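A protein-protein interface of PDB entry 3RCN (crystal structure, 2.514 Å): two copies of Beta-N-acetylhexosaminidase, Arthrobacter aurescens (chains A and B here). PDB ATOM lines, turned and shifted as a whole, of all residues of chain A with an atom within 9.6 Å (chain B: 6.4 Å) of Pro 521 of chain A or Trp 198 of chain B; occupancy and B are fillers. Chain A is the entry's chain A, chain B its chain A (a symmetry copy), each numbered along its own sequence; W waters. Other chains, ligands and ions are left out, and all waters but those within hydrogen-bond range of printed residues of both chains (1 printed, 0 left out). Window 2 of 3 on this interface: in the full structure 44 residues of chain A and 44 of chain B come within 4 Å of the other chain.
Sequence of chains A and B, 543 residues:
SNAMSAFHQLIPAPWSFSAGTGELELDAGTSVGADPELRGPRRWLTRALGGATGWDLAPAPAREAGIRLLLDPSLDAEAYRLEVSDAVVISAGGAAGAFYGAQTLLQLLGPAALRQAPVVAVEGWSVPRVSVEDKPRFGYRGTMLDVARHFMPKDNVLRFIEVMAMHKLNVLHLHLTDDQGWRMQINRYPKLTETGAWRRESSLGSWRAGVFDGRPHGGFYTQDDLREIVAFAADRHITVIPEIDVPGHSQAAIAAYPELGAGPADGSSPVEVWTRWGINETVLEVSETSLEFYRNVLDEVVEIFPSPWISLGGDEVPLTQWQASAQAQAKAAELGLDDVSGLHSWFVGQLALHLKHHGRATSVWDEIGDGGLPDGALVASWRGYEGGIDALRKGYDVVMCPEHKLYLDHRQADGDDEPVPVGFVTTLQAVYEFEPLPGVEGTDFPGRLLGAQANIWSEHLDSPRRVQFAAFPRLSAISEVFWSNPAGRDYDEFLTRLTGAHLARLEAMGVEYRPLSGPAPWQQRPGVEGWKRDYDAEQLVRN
The guanidinium group (NH2) of Arg 465 of chain A is in hydrogen-bond range of the backbone carbonyl oxygen (O) of Gly 218 of chain B (2.7 Å).
O of Trp 522 of chain A sits at hydrogen-bond distance from NH1 of Arg 525 of chain A, at 3.0 Å. The backbone carbonyl oxygen of Gly 219 of chain B sits at hydrogen-bond distance from the guanidinium group of Arg 183 of chain B, 3.1 Å away. The backbone carbonyl oxygen of Glu 194 of chain B lies within hydrogen-bond range of the indole nitrogen of Trp 198 of chain B, at 3.2 Å. The backbone NH of Gly 219 of chain B sits at hydrogen-bond distance from the backbone carbonyl oxygen of Ala 197 of chain B (3.0 Å). N of Arg 199 of chain B sits at hydrogen-bond distance from O of His 217 of chain B, 3.0 Å away.
Among the printed residues, merely in contact across the chains: Arg 465 of chain A with Gly 219 of chain B (3.9 Å), Pro 521 of chain A with Trp 198 of chain B (3.4 Å), Pro 521 of chain A with Pro 216 of chain B (3.7 Å), Trp 522 of chain A with Trp 198 of chain B (3.8 Å), Trp 522 of chain A with His 217 of chain B (3.9 Å), Trp 522 of chain A with Gly 218 of chain B (3.4 Å), Gln 524 of chain A with Pro 216 of chain B (3.5 Å), Arg 525 of chain A with Pro 216 of chain B (3.9 Å) and Pro 526 of chain A with Pro 216 of chain B (3.8 Å).
Gln 523 of chain A touches none of the printed residues of chain B. Of the printed residues of chain B, Gln 524 of chain A touches Pro 216 (3.5 Å). Printed residues of chain B within 4 Å of Pro 526 of chain A: Pro 216 (3.8 Å). Ala 197 of chain B touches none of the printed residues of chain A. Trp 198 of chain B touches just these residues of chain A: Pro 521 and Trp 522. The nearest residue of chain B that does not touch Pro 521 of chain A is Glu 194 of chain B (5.5 Å). The nearest printed residue of chain A that does not touch His 217 of chain B is Arg 465 of chain A (4.03 Å).
Of the 18 printed residues of chain B, 5 touch a printed residue of chain A. Of the 17 printed residues of chain A, 6 touch a printed residue of chain B. Printed residues of chain A that touch a printed residue of chain B: Arg 465, Pro 521, Trp 522, Gln 524, Arg 525 and Pro 526.
No position is printed for both chains. Of the 10 pairs that touch across the chains among the printed residues, none has its exchanged pair printed and touching as well.
Water W1 lies within hydrogen-bond range of NH1 of Arg 465 of chain A, N of Gly 218 of chain B and O of Trp 522 of chain A.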
ATOM      1  N   ASP A 417      35.215  18.180 -19.075  1.00  0.00           N
ATOM      2  CA  ASP A 417      33.888  18.113 -18.466  1.00  0.00           C
ATOM      3  C   ASP A 417      33.719  18.821 -17.118  1.00  0.00           C
ATOM      4  O   ASP A 417      32.597  19.027 -16.660  1.00  0.00           O
ATOM      5  CB  ASP A 417      33.391  16.676 -18.400  1.00  0.00           C
ATOM      6  CG  ASP A 417      32.890  16.189 -19.745  1.00  0.00           C
ATOM      7  OD1 ASP A 417      31.701  16.439 -20.064  1.00  0.00           O
ATOM      8  OD2 ASP A 417      33.690  15.583 -20.494  1.00  0.00           O
ATOM      9  N   PRO A 419      33.573  22.126 -14.844  1.00  0.00           N
ATOM     10  CA  PRO A 419      33.178  23.529 -15.065  1.00  0.00           C
ATOM     11  C   PRO A 419      34.295  24.574 -14.834  1.00  0.00           C
ATOM     12  O   PRO A 419      34.931  24.543 -13.794  1.00  0.00           O
ATOM     13  CB  PRO A 419      32.040  23.735 -14.048  1.00  0.00           C
ATOM     14  CG  PRO A 419      32.257  22.686 -13.004  1.00  0.00           C
ATOM     15  CD  PRO A 419      32.845  21.507 -13.723  1.00  0.00           C
ATOM     16  N   ARG A 465      25.772  27.532  -4.742  1.00  0.00           N
ATOM     17  CA  ARG A 465      25.799  26.171  -5.262  1.00  0.00           C
ATOM     18  C   ARG A 465      27.186  25.868  -5.826  1.00  0.00           C
ATOM     19  O   ARG A 465      27.765  24.819  -5.557  1.00  0.00           O
ATOM     20  CB  ARG A 465      24.733  25.964  -6.337  1.00  0.00           C
ATOM     21  CG  ARG A 465      23.320  26.310  -5.898  1.00  0.00           C
ATOM     22  CD  ARG A 465      22.320  26.157  -7.052  1.00  0.00           C
ATOM     23  NE  ARG A 465      21.967  24.760  -7.264  1.00  0.00           N
ATOM     24  CZ  ARG A 465      21.378  24.284  -8.358  1.00  0.00           C
ATOM     25  NH1 ARG A 465      21.074  25.082  -9.368  1.00  0.00           N
ATOM     26  NH2 ARG A 465      21.106  22.995  -8.442  1.00  0.00           N
ATOM     27  N   PHE A 469      30.017  23.003  -4.771  1.00  0.00           N
ATOM     28  CA  PHE A 469      30.556  22.074  -5.726  1.00  0.00           C
ATOM     29  C   PHE A 469      32.086  22.084  -5.571  1.00  0.00           C
ATOM     30  O   PHE A 469      32.736  21.033  -5.542  1.00  0.00           O
ATOM     31  CB  PHE A 469      30.113  22.492  -7.130  1.00  0.00           C
ATOM     32  CG  PHE A 469      30.707  21.660  -8.226  1.00  0.00           C
ATOM     33  CD1 PHE A 469      31.945  21.983  -8.767  1.00  0.00           C
ATOM     34  CD2 PHE A 469      30.035  20.556  -8.717  1.00  0.00           C
ATOM     35  CE1 PHE A 469      32.498  21.214  -9.775  1.00  0.00           C
ATOM     36  CE2 PHE A 469      30.583  19.789  -9.722  1.00  0.00           C
ATOM     37  CZ  PHE A 469      31.819  20.118 -10.248  1.00  0.00           C
ATOM     38  N   TYR A 513      27.400  18.670  -3.747  1.00  0.00           N
ATOM     39  CA  TYR A 513      28.818  18.435  -3.957  1.00  0.00           C
ATOM     40  C   TYR A 513      29.092  17.932  -5.366  1.00  0.00           C
ATOM     41  O   TYR A 513      28.161  17.720  -6.130  1.00  0.00           O
ATOM     42  CB  TYR A 513      29.293  17.404  -2.938  1.00  0.00           C
ATOM     43  CG  TYR A 513      28.450  16.155  -2.931  1.00  0.00           C
ATOM     44  CD1 TYR A 513      27.370  16.024  -2.055  1.00  0.00           C
ATOM     45  CD2 TYR A 513      28.725  15.110  -3.804  1.00  0.00           C
ATOM     46  CE1 TYR A 513      26.589  14.888  -2.048  1.00  0.00           C
ATOM     47  CE2 TYR A 513      27.957  13.966  -3.809  1.00  0.00           C
ATOM     48  CZ  TYR A 513      26.889  13.857  -2.929  1.00  0.00           C
ATOM     49  OH  TYR A 513      26.133  12.708  -2.940  1.00  0.00           O
ATOM     50  N   ARG A 514      30.365  17.731  -5.714  1.00  0.00           N
ATOM     51  CA  ARG A 514      30.684  17.067  -6.975  1.00  0.00           C
ATOM     52  C   ARG A 514      30.506  15.581  -6.760  1.00  0.00           C
ATOM     53  O   ARG A 514      31.162  15.009  -5.898  1.00  0.00           O
ATOM     54  CB  ARG A 514      32.119  17.327  -7.446  1.00  0.00           C
ATOM     55  CG  ARG A 514      32.320  17.003  -8.940  1.00  0.00           C
ATOM     56  CD  ARG A 514      33.777  17.030  -9.395  1.00  0.00           C
ATOM     57  NE  ARG A 514      34.406  15.729  -9.185  1.00  0.00           N
ATOM     58  CZ  ARG A 514      34.860  14.932 -10.151  1.00  0.00           C
ATOM     59  NH1 ARG A 514      34.790  15.295 -11.426  1.00  0.00           N
ATOM     60  NH2 ARG A 514      35.412  13.769  -9.832  1.00  0.00           N
ATOM     61  N   PRO A 515      29.607  14.949  -7.532  1.00  0.00           N
ATOM     62  CA  PRO A 515      29.480  13.497  -7.406  1.00  0.00           C
ATOM     63  C   PRO A 515      30.795  12.841  -7.793  1.00  0.00           C
ATOM     64  O   PRO A 515      31.523  13.373  -8.632  1.00  0.00           O
ATOM     65  CB  PRO A 515      28.387  13.153  -8.417  1.00  0.00           C
ATOM     66  CG  PRO A 515      27.592  14.408  -8.556  1.00  0.00           C
ATOM     67  CD  PRO A 515      28.628  15.505  -8.482  1.00  0.00           C
ATOM     68  N   SER A 517      31.561  10.411  -9.612  1.00  0.00           N
ATOM     69  CA  SER A 517      31.669  10.025 -11.016  1.00  0.00           C
ATOM     70  C   SER A 517      31.724  11.244 -11.934  1.00  0.00           C
ATOM     71  O   SER A 517      31.746  11.120 -13.149  1.00  0.00           O
ATOM     72  CB  SER A 517      30.557   9.051 -11.422  1.00  0.00           C
ATOM     73  OG  SER A 517      29.270   9.560 -11.116  1.00  0.00           O
ATOM     74  N   GLY A 518      31.771  12.427 -11.345  1.00  0.00           N
ATOM     75  CA  GLY A 518      31.803  13.643 -12.132  1.00  0.00           C
ATOM     76  C   GLY A 518      30.575  14.515 -12.048  1.00  0.00           C
ATOM     77  O   GLY A 518      29.571  14.139 -11.442  1.00  0.00           O
ATOM     78  N   PRO A 519      30.687  15.735 -12.581  1.00  0.00           N
ATOM     79  CA  PRO A 519      29.647  16.761 -12.472  1.00  0.00           C
ATOM     80  C   PRO A 519      28.297  16.326 -13.024  1.00  0.00           C
ATOM     81  O   PRO A 519      28.235  15.702 -14.085  1.00  0.00           O
ATOM     82  CB  PRO A 519      30.210  17.930 -13.298  1.00  0.00           C
ATOM     83  CG  PRO A 519      31.409  17.377 -14.029  1.00  0.00           C
ATOM     84  CD  PRO A 519      31.916  16.261 -13.198  1.00  0.00           C
ATOM     85  N   ALA A 520      27.231  16.657 -12.295  1.00  0.00           N
ATOM     86  CA  ALA A 520      25.877  16.511 -12.809  1.00  0.00           C
ATOM     87  C   ALA A 520      25.712  17.475 -13.965  1.00  0.00           C
ATOM     88  O   ALA A 520      26.328  18.529 -13.986  1.00  0.00           O
ATOM     89  CB  ALA A 520      24.851  16.797 -11.718  1.00  0.00           C
ATOM     90  N   PRO A 521      24.885  17.115 -14.945  1.00  0.00           N
ATOM     91  CA  PRO A 521      24.711  17.957 -16.131  1.00  0.00           C
ATOM     92  C   PRO A 521      24.403  19.425 -15.808  1.00  0.00           C
ATOM     93  O   PRO A 521      24.844  20.291 -16.558  1.00  0.00           O
ATOM     94  CB  PRO A 521      23.516  17.301 -16.836  1.00  0.00           C
ATOM     95  CG  PRO A 521      23.616  15.863 -16.444  1.00  0.00           C
ATOM     96  CD  PRO A 521      24.094  15.874 -15.020  1.00  0.00           C
ATOM     97  N   TRP A 522      23.653  19.702 -14.740  1.00  0.00           N
ATOM     98  CA  TRP A 522      23.321  21.089 -14.399  1.00  0.00           C
ATOM     99  C   TRP A 522      24.473  21.808 -13.699  1.00  0.00           C
ATOM    100  O   TRP A 522      24.432  23.015 -13.493  1.00  0.00           O
ATOM    101  CB  TRP A 522      22.040  21.185 -13.555  1.00  0.00           C
ATOM    102  CG  TRP A 522      22.090  20.421 -12.277  1.00  0.00           C
ATOM    103  CD1 TRP A 522      22.528  20.871 -11.058  1.00  0.00           C
ATOM    104  CD2 TRP A 522      21.686  19.063 -12.081  1.00  0.00           C
ATOM    105  NE1 TRP A 522      22.422  19.868 -10.115  1.00  0.00           N
ATOM    106  CE2 TRP A 522      21.907  18.750 -10.723  1.00  0.00           C
ATOM    107  CE3 TRP A 522      21.169  18.077 -12.922  1.00  0.00           C
ATOM    108  CZ2 TRP A 522      21.628  17.492 -10.195  1.00  0.00           C
ATOM    109  CZ3 TRP A 522      20.884  16.826 -12.392  1.00  0.00           C
ATOM    110  CH2 TRP A 522      21.115  16.547 -11.044  1.00  0.00           C
ATOM    111  N   GLN A 523      25.485  21.047 -13.313  1.00  0.00           N
ATOM    112  CA  GLN A 523      26.696  21.597 -12.715  1.00  0.00           C
ATOM    113  C   GLN A 523      27.752  21.978 -13.746  1.00  0.00           C
ATOM    114  O   GLN A 523      28.729  22.646 -13.423  1.00  0.00           O
ATOM    115  CB  GLN A 523      27.300  20.586 -11.746  1.00  0.00           C
ATOM    116  CG  GLN A 523      26.495  20.397 -10.474  1.00  0.00           C
ATOM    117  CD  GLN A 523      26.972  19.193  -9.703  1.00  0.00           C
ATOM    118  OE1 GLN A 523      27.632  18.307 -10.259  1.00  0.00           O
ATOM    119  NE2 GLN A 523      26.660  19.154  -8.415  1.00  0.00           N
ATOM    120  N   GLN A 524      27.574  21.538 -14.981  1.00  0.00           N
ATOM    121  CA  GLN A 524      28.518  21.875 -16.030  1.00  0.00           C
ATOM    122  C   GLN A 524      28.343  23.308 -16.563  1.00  0.00           C
ATOM    123  O   GLN A 524      27.287  23.914 -16.424  1.00  0.00           O
ATOM    124  CB  GLN A 524      28.438  20.836 -17.142  1.00  0.00           C
ATOM    125  CG  GLN A 524      28.989  19.501 -16.710  1.00  0.00           C
ATOM    126  CD  GLN A 524      28.745  18.424 -17.732  1.00  0.00           C
ATOM    127  OE1 GLN A 524      28.746  18.689 -18.935  1.00  0.00           O
ATOM    128  NE2 GLN A 524      28.517  17.198 -17.261  1.00  0.00           N
ATOM    129  N   ARG A 525      29.401  23.857 -17.139  1.00  0.00           N
ATOM    130  CA  ARG A 525      29.332  25.187 -17.729  1.00  0.00           C
ATOM    131  C   ARG A 525      30.156  25.216 -19.015  1.00  0.00           C
ATOM    132  O   ARG A 525      31.261  25.747 -19.038  1.00  0.00           O
ATOM    133  CB  ARG A 525      29.854  26.249 -16.749  1.00  0.00           C
ATOM    134  CG  ARG A 525      29.151  26.270 -15.386  1.00  0.00           C
ATOM    135  CD  ARG A 525      27.979  27.258 -15.323  1.00  0.00           C
ATOM    136  NE  ARG A 525      27.360  27.299 -13.993  1.00  0.00           N
ATOM    137  CZ  ARG A 525      26.498  26.393 -13.528  1.00  0.00           C
ATOM    138  NH1 ARG A 525      26.145  25.357 -14.280  1.00  0.00           N
ATOM    139  NH2 ARG A 525      25.992  26.511 -12.306  1.00  0.00           N
ATOM    140  N   PRO A 526      29.629  24.624 -20.085  1.00  0.00           N
ATOM    141  CA  PRO A 526      30.329  24.582 -21.376  1.00  0.00           C
ATOM    142  C   PRO A 526      30.456  25.954 -22.036  1.00  0.00           C
ATOM    143  O   PRO A 526      29.613  26.828 -21.832  1.00  0.00           O
ATOM    144  CB  PRO A 526      29.435  23.675 -22.231  1.00  0.00           C
ATOM    145  CG  PRO A 526      28.045  23.770 -21.592  1.00  0.00           C
ATOM    146  CD  PRO A 526      28.314  23.947 -20.119  1.00  0.00           C
ATOM    147  N   GLN B 180      10.021  23.752 -18.255  1.00  0.00           N
ATOM    148  CA  GLN B 180      11.459  24.026 -18.148  1.00  0.00           C
ATOM    149  C   GLN B 180      12.213  23.244 -17.075  1.00  0.00           C
ATOM    150  O   GLN B 180      13.395  23.453 -16.891  1.00  0.00           O
ATOM    151  CB  GLN B 180      11.691  25.523 -17.968  1.00  0.00           C
ATOM    152  CG  GLN B 180      11.069  26.344 -19.089  1.00  0.00           C
ATOM    153  CD  GLN B 180       9.631  26.766 -18.812  1.00  0.00           C
ATOM    154  OE1 GLN B 180       8.998  26.312 -17.855  1.00  0.00           O
ATOM    155  NE2 GLN B 180       9.116  27.649 -19.651  1.00  0.00           N
ATOM    156  N   GLY B 181      11.512  22.378 -16.353  1.00  0.00           N
ATOM    157  CA  GLY B 181      12.127  21.449 -15.422  1.00  0.00           C
ATOM    158  C   GLY B 181      11.097  20.759 -14.535  1.00  0.00           C
ATOM    159  O   GLY B 181       9.987  21.256 -14.373  1.00  0.00           O
ATOM    160  N   TRP B 182      11.503  19.643 -13.931  1.00  0.00           N
ATOM    161  CA  TRP B 182      10.703  18.843 -13.012  1.00  0.00           C
ATOM    162  C   TRP B 182      11.527  18.640 -11.720  1.00  0.00           C
ATOM    163  O   TRP B 182      12.613  18.059 -11.751  1.00  0.00           O
ATOM    164  CB  TRP B 182      10.376  17.495 -13.666  1.00  0.00           C
ATOM    165  CG  TRP B 182       9.587  16.551 -12.776  1.00  0.00           C
ATOM    166  CD1 TRP B 182      10.047  15.890 -11.677  1.00  0.00           C
ATOM    167  CD2 TRP B 182       8.210  16.164 -12.930  1.00  0.00           C
ATOM    168  NE1 TRP B 182       9.043  15.131 -11.127  1.00  0.00           N
ATOM    169  CE2 TRP B 182       7.907  15.280 -11.876  1.00  0.00           C
ATOM    170  CE3 TRP B 182       7.205  16.485 -13.855  1.00  0.00           C
ATOM    171  CZ2 TRP B 182       6.638  14.713 -11.715  1.00  0.00           C
ATOM    172  CZ3 TRP B 182       5.946  15.920 -13.697  1.00  0.00           C
ATOM    173  CH2 TRP B 182       5.670  15.051 -12.627  1.00  0.00           C
ATOM    174  N   ARG B 183      11.040  19.165 -10.595  1.00  0.00           N
ATOM    175  CA  ARG B 183      11.847  19.227  -9.376  1.00  0.00           C
ATOM    176  C   ARG B 183      11.622  18.114  -8.363  1.00  0.00           C
ATOM    177  O   ARG B 183      12.274  18.072  -7.320  1.00  0.00           O
ATOM    178  CB  ARG B 183      11.655  20.568  -8.670  1.00  0.00           C
ATOM    179  CG  ARG B 183      11.921  21.780  -9.519  1.00  0.00           C
ATOM    180  CD  ARG B 183      13.243  21.709 -10.228  1.00  0.00           C
ATOM    181  NE  ARG B 183      13.397  22.843 -11.130  1.00  0.00           N
ATOM    182  CZ  ARG B 183      14.249  22.858 -12.149  1.00  0.00           C
ATOM    183  NH1 ARG B 183      15.010  21.797 -12.370  1.00  0.00           N
ATOM    184  NH2 ARG B 183      14.335  23.917 -12.948  1.00  0.00           N
ATOM    185  N   LEU B 192      12.374  11.285 -14.516  1.00  0.00           N
ATOM    186  CA  LEU B 192      11.732  12.569 -14.257  1.00  0.00           C
ATOM    187  C   LEU B 192      12.776  13.555 -13.764  1.00  0.00           C
ATOM    188  O   LEU B 192      12.817  14.713 -14.200  1.00  0.00           O
ATOM    189  CB  LEU B 192      10.580  12.435 -13.259  1.00  0.00           C
ATOM    190  CG  LEU B 192       9.282  11.948 -13.930  1.00  0.00           C
ATOM    191  CD1 LEU B 192       8.097  11.890 -12.958  1.00  0.00           C
ATOM    192  CD2 LEU B 192       8.932  12.812 -15.153  1.00  0.00           C
ATOM    193  N   THR B 193      13.581  13.105 -12.806  1.00  0.00           N
ATOM    194  CA  THR B 193      14.722  13.884 -12.350  1.00  0.00           C
ATOM    195  C   THR B 193      15.998  13.734 -13.198  1.00  0.00           C
ATOM    196  O   THR B 193      16.647  14.731 -13.505  1.00  0.00           O
ATOM    197  CB  THR B 193      14.981  13.680 -10.857  1.00  0.00           C
ATOM    198  OG1 THR B 193      15.144  12.282 -10.587  1.00  0.00           O
ATOM    199  CG2 THR B 193      13.790  14.218 -10.058  1.00  0.00           C
ATOM    200  N   GLU B 194      16.342  12.510 -13.601  1.00  0.00           N
ATOM    201  CA  GLU B 194      17.571  12.295 -14.375  1.00  0.00           C
ATOM    202  C   GLU B 194      17.604  13.114 -15.664  1.00  0.00           C
ATOM    203  O   GLU B 194      18.623  13.678 -16.040  1.00  0.00           O
ATOM    204  CB  GLU B 194      17.769  10.820 -14.707  1.00  0.00           C
ATOM    205  CG  GLU B 194      18.125   9.944 -13.525  1.00  0.00           C
ATOM    206  CD  GLU B 194      18.071   8.456 -13.865  1.00  0.00           C
ATOM    207  OE1 GLU B 194      17.938   8.115 -15.066  1.00  0.00           O
ATOM    208  OE2 GLU B 194      18.152   7.629 -12.927  1.00  0.00           O
ATOM    209  N   THR B 195      16.470  13.169 -16.331  1.00  0.00           N
ATOM    210  CA  THR B 195      16.317  13.885 -17.587  1.00  0.00           C
ATOM    211  C   THR B 195      15.589  15.201 -17.323  1.00  0.00           C
ATOM    212  O   THR B 195      16.072  16.258 -17.699  1.00  0.00           O
ATOM    213  CB  THR B 195      15.642  13.014 -18.684  1.00  0.00           C
ATOM    214  OG1 THR B 195      16.524  11.938 -19.033  1.00  0.00           O
ATOM    215  CG2 THR B 195      15.349  13.827 -19.938  1.00  0.00           C
ATOM    216  N   GLY B 196      14.380  15.113 -16.772  1.00  0.00           N
ATOM    217  CA  GLY B 196      13.547  16.276 -16.513  1.00  0.00           C
ATOM    218  C   GLY B 196      14.035  17.343 -15.540  1.00  0.00           C
ATOM    219  O   GLY B 196      13.502  18.457 -15.533  1.00  0.00           O
ATOM    220  N   ALA B 197      15.049  17.041 -14.734  1.00  0.00           N
ATOM    221  CA  ALA B 197      15.485  17.992 -13.704  1.00  0.00           C
ATOM    222  C   ALA B 197      16.490  19.040 -14.174  1.00  0.00           C
ATOM    223  O   ALA B 197      16.961  19.845 -13.361  1.00  0.00           O
ATOM    224  CB  ALA B 197      16.020  17.270 -12.486  1.00  0.00           C
ATOM    225  N   TRP B 198      16.840  19.020 -15.462  1.00  0.00           N
ATOM    226  CA  TRP B 198      17.781  20.009 -16.003  1.00  0.00           C
ATOM    227  C   TRP B 198      17.513  20.360 -17.458  1.00  0.00           C
ATOM    228  O   TRP B 198      16.985  19.551 -18.210  1.00  0.00           O
ATOM    229  CB  TRP B 198      19.240  19.544 -15.834  1.00  0.00           C
ATOM    230  CG  TRP B 198      19.629  18.375 -16.703  1.00  0.00           C
ATOM    231  CD1 TRP B 198      19.385  17.055 -16.452  1.00  0.00           C
ATOM    232  CD2 TRP B 198      20.343  18.419 -17.956  1.00  0.00           C
ATOM    233  NE1 TRP B 198      19.896  16.276 -17.465  1.00  0.00           N
ATOM    234  CE2 TRP B 198      20.487  17.084 -18.397  1.00  0.00           C
ATOM    235  CE3 TRP B 198      20.863  19.452 -18.740  1.00  0.00           C
ATOM    236  CZ2 TRP B 198      21.142  16.753 -19.602  1.00  0.00           C
ATOM    237  CZ3 TRP B 198      21.515  19.120 -19.933  1.00  0.00           C
ATOM    238  CH2 TRP B 198      21.642  17.779 -20.349  1.00  0.00           C
ATOM    239  N   ARG B 199      17.891  21.573 -17.843  1.00  0.00           N
ATOM    240  CA  ARG B 199      17.793  22.022 -19.224  1.00  0.00           C
ATOM    241  C   ARG B 199      19.153  22.555 -19.693  1.00  0.00           C
ATOM    242  O   ARG B 199      19.976  22.950 -18.876  1.00  0.00           O
ATOM    243  CB  ARG B 199      16.738  23.126 -19.354  1.00  0.00           C
ATOM    244  CG  ARG B 199      17.046  24.377 -18.553  1.00  0.00           C
ATOM    245  CD  ARG B 199      15.927  25.389 -18.680  1.00  0.00           C
ATOM    246  NE  ARG B 199      16.140  26.567 -17.842  1.00  0.00           N
ATOM    247  CZ  ARG B 199      15.618  26.727 -16.626  1.00  0.00           C
ATOM    248  NH1 ARG B 199      14.850  25.777 -16.085  1.00  0.00           N
ATOM    249  NH2 ARG B 199      15.868  27.842 -15.944  1.00  0.00           N
ATOM    250  N   ARG B 200      19.360  22.569 -21.008  1.00  0.00           N
ATOM    251  CA  ARG B 200      20.592  23.019 -21.654  1.00  0.00           C
ATOM    252  C   ARG B 200      20.910  24.489 -21.389  1.00  0.00           C
ATOM    253  O   ARG B 200      22.052  24.851 -21.082  1.00  0.00           O
ATOM    254  CB  ARG B 200      20.451  22.842 -23.160  1.00  0.00           C
ATOM    255  CG  ARG B 200      21.608  22.161 -23.811  1.00  0.00           C
ATOM    256  CD  ARG B 200      21.201  20.788 -24.300  1.00  0.00           C
ATOM    257  NE  ARG B 200      22.313  19.846 -24.212  1.00  0.00           N
ATOM    258  CZ  ARG B 200      22.181  18.529 -24.299  1.00  0.00           C
ATOM    259  NH1 ARG B 200      20.978  17.997 -24.472  1.00  0.00           N
ATOM    260  NH2 ARG B 200      23.252  17.747 -24.205  1.00  0.00           N
ATOM    261  N   PRO B 216      23.605  25.843 -18.573  1.00  0.00           N
ATOM    262  CA  PRO B 216      22.767  24.774 -18.041  1.00  0.00           C
ATOM    263  C   PRO B 216      22.126  25.206 -16.723  1.00  0.00           C
ATOM    264  O   PRO B 216      22.734  25.975 -15.972  1.00  0.00           O
ATOM    265  CB  PRO B 216      23.773  23.648 -17.795  1.00  0.00           C
ATOM    266  CG  PRO B 216      24.780  23.836 -18.853  1.00  0.00           C
ATOM    267  CD  PRO B 216      24.919  25.342 -19.008  1.00  0.00           C
ATOM    268  N   HIS B 217      20.898  24.755 -16.467  1.00  0.00           N
ATOM    269  CA  HIS B 217      20.275  24.983 -15.166  1.00  0.00           C
ATOM    270  C   HIS B 217      19.443  23.800 -14.695  1.00  0.00           C
ATOM    271  O   HIS B 217      18.726  23.180 -15.484  1.00  0.00           O
ATOM    272  CB  HIS B 217      19.417  26.252 -15.145  1.00  0.00           C
ATOM    273  CG  HIS B 217      18.697  26.435 -13.846  1.00  0.00           C
ATOM    274  ND1 HIS B 217      19.290  27.008 -12.742  1.00  0.00           N
ATOM    275  CD2 HIS B 217      17.464  26.034 -13.447  1.00  0.00           C
ATOM    276  CE1 HIS B 217      18.437  26.999 -11.732  1.00  0.00           C
ATOM    277  NE2 HIS B 217      17.323  26.409 -12.133  1.00  0.00           N
ATOM    278  N   GLY B 218      19.523  23.499 -13.403  1.00  0.00           N
ATOM    279  CA  GLY B 218      18.731  22.419 -12.853  1.00  0.00           C
ATOM    280  C   GLY B 218      18.974  22.073 -11.399  1.00  0.00           C
ATOM    281  O   GLY B 218      19.680  22.769 -10.672  1.00  0.00           O
ATOM    282  N   GLY B 219      18.299  21.015 -10.964  1.00  0.00           N
ATOM    283  CA  GLY B 219      18.420  20.475  -9.622  1.00  0.00           C
ATOM    284  C   GLY B 219      17.069  19.863  -9.279  1.00  0.00           C
ATOM    285  O   GLY B 219      16.113  19.993 -10.043  1.00  0.00           O
ATOM    286  N   VAL B 273      14.020  19.021 -22.378  1.00  0.00           N
ATOM    287  CA  VAL B 273      13.423  19.983 -21.448  1.00  0.00           C
ATOM    288  C   VAL B 273      13.377  21.360 -22.132  1.00  0.00           C
ATOM    289  O   VAL B 273      14.333  21.755 -22.792  1.00  0.00           O
ATOM    290  CB  VAL B 273      14.196  20.062 -20.110  1.00  0.00           C
ATOM    291  CG1 VAL B 273      13.558  21.090 -19.193  1.00  0.00           C
ATOM    292  CG2 VAL B 273      14.233  18.711 -19.418  1.00  0.00           C
HETATM  293  O   HOH W   1      21.998  24.845 -12.142  1.00  0.00           O
